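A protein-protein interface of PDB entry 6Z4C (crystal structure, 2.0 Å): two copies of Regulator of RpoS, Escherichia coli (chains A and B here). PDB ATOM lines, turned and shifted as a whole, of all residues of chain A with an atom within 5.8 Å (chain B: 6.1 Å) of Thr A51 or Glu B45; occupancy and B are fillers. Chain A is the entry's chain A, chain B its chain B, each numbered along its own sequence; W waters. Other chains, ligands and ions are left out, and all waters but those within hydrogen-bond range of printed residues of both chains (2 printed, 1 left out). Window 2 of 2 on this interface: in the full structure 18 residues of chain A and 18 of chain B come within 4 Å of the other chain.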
ATOM      1  N   GLN A   9      16.548   2.270  23.138  1.00  0.00           N
ATOM      2  CA  GLN A   9      18.002   1.946  23.145  1.00  0.00           C
ATOM      3  C   GLN A   9      18.461   1.955  24.606  1.00  0.00           C
ATOM      4  O   GLN A   9      18.291   2.995  25.294  1.00  0.00           O
ATOM      5  CB  GLN A   9      18.793   2.942  22.295  1.00  0.00           C
ATOM      6  CG  GLN A   9      18.199   3.192  20.913  1.00  0.00           C
ATOM      7  CD  GLN A   9      19.028   4.108  20.034  1.00  0.00           C
ATOM      8  OE1 GLN A   9      19.074   5.326  20.189  1.00  0.00           O
ATOM      9  NE2 GLN A   9      19.737   3.503  19.099  1.00  0.00           N
ATOM     10  N   LEU A  47      29.770   6.907  24.981  1.00  0.00           N
ATOM     11  CA  LEU A  47      28.743   7.973  25.196  1.00  0.00           C
ATOM     12  C   LEU A  47      29.181   9.285  24.548  1.00  0.00           C
ATOM     13  O   LEU A  47      28.359  10.211  24.493  1.00  0.00           O
ATOM     14  CB  LEU A  47      28.472   8.155  26.688  1.00  0.00           C
ATOM     15  CG  LEU A  47      27.535   7.095  27.244  1.00  0.00           C
ATOM     16  CD1 LEU A  47      27.673   6.945  28.737  1.00  0.00           C
ATOM     17  CD2 LEU A  47      26.111   7.381  26.853  1.00  0.00           C
ATOM     18  N   GLY A  49      29.628   9.565  21.426  1.00  0.00           N
ATOM     19  CA  GLY A  49      29.013   9.585  20.081  1.00  0.00           C
ATOM     20  C   GLY A  49      27.600   9.033  20.026  1.00  0.00           C
ATOM     21  O   GLY A  49      27.025   9.016  18.947  1.00  0.00           O
ATOM     22  N   PHE A  50      27.055   8.557  21.133  1.00  0.00           N
ATOM     23  CA  PHE A  50      25.815   7.755  21.154  1.00  0.00           C
ATOM     24  C   PHE A  50      25.002   8.242  22.342  1.00  0.00           C
ATOM     25  O   PHE A  50      25.622   8.448  23.405  1.00  0.00           O
ATOM     26  CB  PHE A  50      26.248   6.300  21.268  1.00  0.00           C
ATOM     27  CG  PHE A  50      25.185   5.341  21.699  1.00  0.00           C
ATOM     28  CD1 PHE A  50      24.216   4.901  20.809  1.00  0.00           C
ATOM     29  CD2 PHE A  50      25.197   4.827  22.974  1.00  0.00           C
ATOM     30  CE1 PHE A  50      23.249   3.997  21.205  1.00  0.00           C
ATOM     31  CE2 PHE A  50      24.227   3.928  23.366  1.00  0.00           C
ATOM     32  CZ  PHE A  50      23.271   3.506  22.485  1.00  0.00           C
ATOM     33  N   THR A  51      23.687   8.370  22.192  1.00  0.00           N
ATOM     34  CA  THR A  51      22.767   8.812  23.265  1.00  0.00           C
ATOM     35  C   THR A  51      21.684   7.743  23.461  1.00  0.00           C
ATOM     36  O   THR A  51      20.671   7.718  22.782  1.00  0.00           O
ATOM     37  CB  THR A  51      22.193  10.197  22.924  1.00  0.00           C
ATOM     38  OG1 THR A  51      21.509  10.126  21.668  1.00  0.00           O
ATOM     39  CG2 THR A  51      23.262  11.262  22.789  1.00  0.00           C
ATOM     40  N   PRO A  52      21.809   6.843  24.445  1.00  0.00           N
ATOM     41  CA  PRO A  52      20.752   5.863  24.719  1.00  0.00           C
ATOM     42  C   PRO A  52      19.497   6.457  25.387  1.00  0.00           C
ATOM     43  O   PRO A  52      19.554   7.544  25.883  1.00  0.00           O
ATOM     44  CB  PRO A  52      21.428   4.905  25.686  1.00  0.00           C
ATOM     45  CG  PRO A  52      22.431   5.758  26.400  1.00  0.00           C
ATOM     46  CD  PRO A  52      22.909   6.784  25.391  1.00  0.00           C
ATOM     47  N   ASP A  53      18.417   5.688  25.463  1.00  0.00           N
ATOM     48  CA  ASP A  53      17.188   6.110  26.184  1.00  0.00           C
ATOM     49  C   ASP A  53      17.405   5.921  27.688  1.00  0.00           C
ATOM     50  O   ASP A  53      16.819   6.678  28.480  1.00  0.00           O
ATOM     51  CB  ASP A  53      15.967   5.399  25.591  1.00  0.00           C
ATOM     52  CG  ASP A  53      15.797   5.784  24.127  1.00  0.00           C
ATOM     53  OD1 ASP A  53      15.676   6.983  23.883  1.00  0.00           O
ATOM     54  OD2 ASP A  53      15.849   4.903  23.249  1.00  0.00           O
ATOM     55  N   ASP A  78      24.897  16.075  29.533  1.00  0.00           N
ATOM     56  CA  ASP A  78      24.043  14.890  29.230  1.00  0.00           C
ATOM     57  C   ASP A  78      22.909  14.789  30.248  1.00  0.00           C
ATOM     58  O   ASP A  78      23.199  14.768  31.455  1.00  0.00           O
ATOM     59  CB  ASP A  78      24.791  13.562  29.336  1.00  0.00           C
ATOM     60  CG  ASP A  78      25.530  13.200  28.073  1.00  0.00           C
ATOM     61  OD1 ASP A  78      26.035  14.148  27.401  1.00  0.00           O
ATOM     62  OD2 ASP A  78      25.582  11.976  27.768  1.00  0.00           O
ATOM     63  N   THR A  80      20.945  12.051  29.853  1.00  0.00           N
ATOM     64  CA  THR A  80      20.708  10.591  29.706  1.00  0.00           C
ATOM     65  C   THR A  80      20.177  10.052  31.032  1.00  0.00           C
ATOM     66  O   THR A  80      20.847  10.102  32.048  1.00  0.00           O
ATOM     67  CB  THR A  80      21.981   9.817  29.340  1.00  0.00           C
ATOM     68  OG1 THR A  80      22.465  10.342  28.113  1.00  0.00           O
ATOM     69  CG2 THR A  80      21.759   8.326  29.204  1.00  0.00           C
ATOM     70  N   GLY B  40      22.712  -3.192  14.048  1.00  0.00           N
ATOM     71  CA  GLY B  40      23.809  -2.703  13.200  1.00  0.00           C
ATOM     72  C   GLY B  40      23.777  -1.192  13.014  1.00  0.00           C
ATOM     73  O   GLY B  40      24.873  -0.553  12.895  1.00  0.00           O
ATOM     74  N   VAL B  41      22.589  -0.595  13.033  1.00  0.00           N
ATOM     75  CA  VAL B  41      22.474   0.886  12.979  1.00  0.00           C
ATOM     76  C   VAL B  41      23.088   1.482  14.260  1.00  0.00           C
ATOM     77  O   VAL B  41      23.837   2.458  14.146  1.00  0.00           O
ATOM     78  CB  VAL B  41      21.026   1.345  12.777  1.00  0.00           C
ATOM     79  CG1 VAL B  41      20.951   2.864  12.735  1.00  0.00           C
ATOM     80  CG2 VAL B  41      20.432   0.718  11.525  1.00  0.00           C
ATOM     81  N   ASP B  42      22.799   0.905  15.415  1.00  0.00           N
ATOM     82  CA  ASP B  42      23.378   1.322  16.718  1.00  0.00           C
ATOM     83  C   ASP B  42      24.914   1.196  16.680  1.00  0.00           C
ATOM     84  O   ASP B  42      25.570   2.167  17.125  1.00  0.00           O
ATOM     85  CB  ASP B  42      22.837   0.518  17.888  1.00  0.00           C
ATOM     86  CG  ASP B  42      21.390   0.795  18.258  1.00  0.00           C
ATOM     87  OD1 ASP B  42      20.804   1.759  17.706  1.00  0.00           O
ATOM     88  OD2 ASP B  42      20.856   0.030  19.110  1.00  0.00           O
ATOM     89  N   ALA B  43      25.455   0.100  16.121  1.00  0.00           N
ATOM     90  CA  ALA B  43      26.920  -0.097  15.944  1.00  0.00           C
ATOM     91  C   ALA B  43      27.506   1.027  15.063  1.00  0.00           C
ATOM     92  O   ALA B  43      28.525   1.620  15.442  1.00  0.00           O
ATOM     93  CB  ALA B  43      27.205  -1.461  15.345  1.00  0.00           C
ATOM     94  N   LEU B  44      26.871   1.331  13.930  1.00  0.00           N
ATOM     95  CA  LEU B  44      27.274   2.479  13.082  1.00  0.00           C
ATOM     96  C   LEU B  44      27.383   3.739  13.935  1.00  0.00           C
ATOM     97  O   LEU B  44      28.416   4.418  13.872  1.00  0.00           O
ATOM     98  CB  LEU B  44      26.303   2.672  11.908  1.00  0.00           C
ATOM     99  CG  LEU B  44      26.697   3.769  10.918  1.00  0.00           C
ATOM    100  CD1 LEU B  44      28.078   3.526  10.338  1.00  0.00           C
ATOM    101  CD2 LEU B  44      25.696   3.849   9.791  1.00  0.00           C
ATOM    102  N   GLU B  45      26.355   4.050  14.705  1.00  0.00           N
ATOM    103  CA  GLU B  45      26.346   5.227  15.611  1.00  0.00           C
ATOM    104  C   GLU B  45      27.528   5.112  16.591  1.00  0.00           C
ATOM    105  O   GLU B  45      28.298   6.084  16.681  1.00  0.00           O
ATOM    106  CB  GLU B  45      24.974   5.370  16.288  1.00  0.00           C
ATOM    107  CG  GLU B  45      24.793   6.675  17.040  1.00  0.00           C
ATOM    108  CD  GLU B  45      23.484   6.777  17.811  1.00  0.00           C
ATOM    109  OE1 GLU B  45      22.676   5.839  17.724  1.00  0.00           O
ATOM    110  OE2 GLU B  45      23.270   7.797  18.517  1.00  0.00           O
ATOM    111  N   LEU B  46      27.739   3.966  17.249  1.00  0.00           N
ATOM    112  CA  LEU B  46      28.805   3.838  18.272  1.00  0.00           C
ATOM    113  C   LEU B  46      30.159   4.153  17.650  1.00  0.00           C
ATOM    114  O   LEU B  46      31.022   4.672  18.352  1.00  0.00           O
ATOM    115  CB  LEU B  46      28.864   2.412  18.840  1.00  0.00           C
ATOM    116  CG  LEU B  46      27.637   1.941  19.582  1.00  0.00           C
ATOM    117  CD1 LEU B  46      27.797   0.491  19.967  1.00  0.00           C
ATOM    118  CD2 LEU B  46      27.399   2.809  20.802  1.00  0.00           C
ATOM    119  N   LEU B  47      30.387   3.721  16.416  1.00  0.00           N
ATOM    120  CA  LEU B  47      31.713   3.808  15.754  1.00  0.00           C
ATOM    121  C   LEU B  47      32.037   5.262  15.415  1.00  0.00           C
ATOM    122  O   LEU B  47      33.190   5.539  15.114  1.00  0.00           O
ATOM    123  CB  LEU B  47      31.740   2.902  14.520  1.00  0.00           C
ATOM    124  CG  LEU B  47      31.987   1.443  14.858  1.00  0.00           C
ATOM    125  CD1 LEU B  47      31.649   0.535  13.703  1.00  0.00           C
ATOM    126  CD2 LEU B  47      33.415   1.251  15.313  1.00  0.00           C
ATOM    127  N   GLY B  48      31.062   6.160  15.501  1.00  0.00           N
ATOM    128  CA  GLY B  48      31.318   7.602  15.416  1.00  0.00           C
ATOM    129  C   GLY B  48      32.316   8.023  16.491  1.00  0.00           C
ATOM    130  O   GLY B  48      33.226   8.798  16.151  1.00  0.00           O
ATOM    131  N   GLY B  49      32.200   7.515  17.728  1.00  0.00           N
ATOM    132  CA  GLY B  49      33.008   8.017  18.867  1.00  0.00           C
ATOM    133  C   GLY B  49      34.037   7.039  19.419  1.00  0.00           C
ATOM    134  O   GLY B  49      34.770   7.401  20.350  1.00  0.00           O
HETATM  135  O   HOH W   1      30.344   6.592  20.147  1.00  0.00           O
HETATM  136  O   HOH W   2      17.791   1.378  17.324  1.00  0.00           O
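Positions printed for both chains: 47 and 49.
Of the 6 pairs that touch across the chains among the printed residues, none has its exchanged pair printed and touching as well.
Water W1 lies within hydrogen-bond range of the backbone carbonyl oxygen of Leu B46 (2.7 Å), the backbone NH of Gly B49 (3.2 Å) and the backbone NH of Gly A49 (3.3 Å).
Water W2 bridges the side-chain carboxylate of Asp B42 (3.1 Å) and the side-chain amide nitrogen of Gln A9 (3.4 Å).
Among the printed residues, pairs that only touch across the chains: Gln A9 with Glu B45 (3.998 Å), Gly A49 with Glu B45 (3.8 Å), Phe A50 with Glu B45 (3.6 Å), Phe A50 with Leu B46 (3.5 Å) and Thr A51 with Glu B45 (3.7 Å).
Of the 9 printed residues of chain A, 4 touch a printed residue of chain B.
Among the printed residues, 6 pairs touch across the chains.
The side-chain amide nitrogen (NE2) of Gln A9 is in hydrogen-bond range of the side-chain carboxylate (OD1) of Asp B42 (2.5 Å).
O of Gln A9 sits at hydrogen-bond distance from N of Asp A53.
Thr A51 touches just one residue of chain B: Glu B45.
Of the printed residues of chain A, Glu B45 touches Gln A9 (3.998 Å), Gly A49 (3.8 Å), Phe A50 (3.6 Å) and Thr A51 (3.7 Å).
Of the printed residues of chain B, Gly A49 touches Glu B45.
Of the printed residues of chain B, Phe A50 touches Glu B45 (3.6 Å) and Leu B46 (3.5 Å).
Printed residues of chain A within 4 Å of Asp B42: Gln A9.
Asp A78 touches none of the printed residues of chain B.
The nearest printed residue of chain B that does not touch Thr A51 is Leu B46 (6.8 Å).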
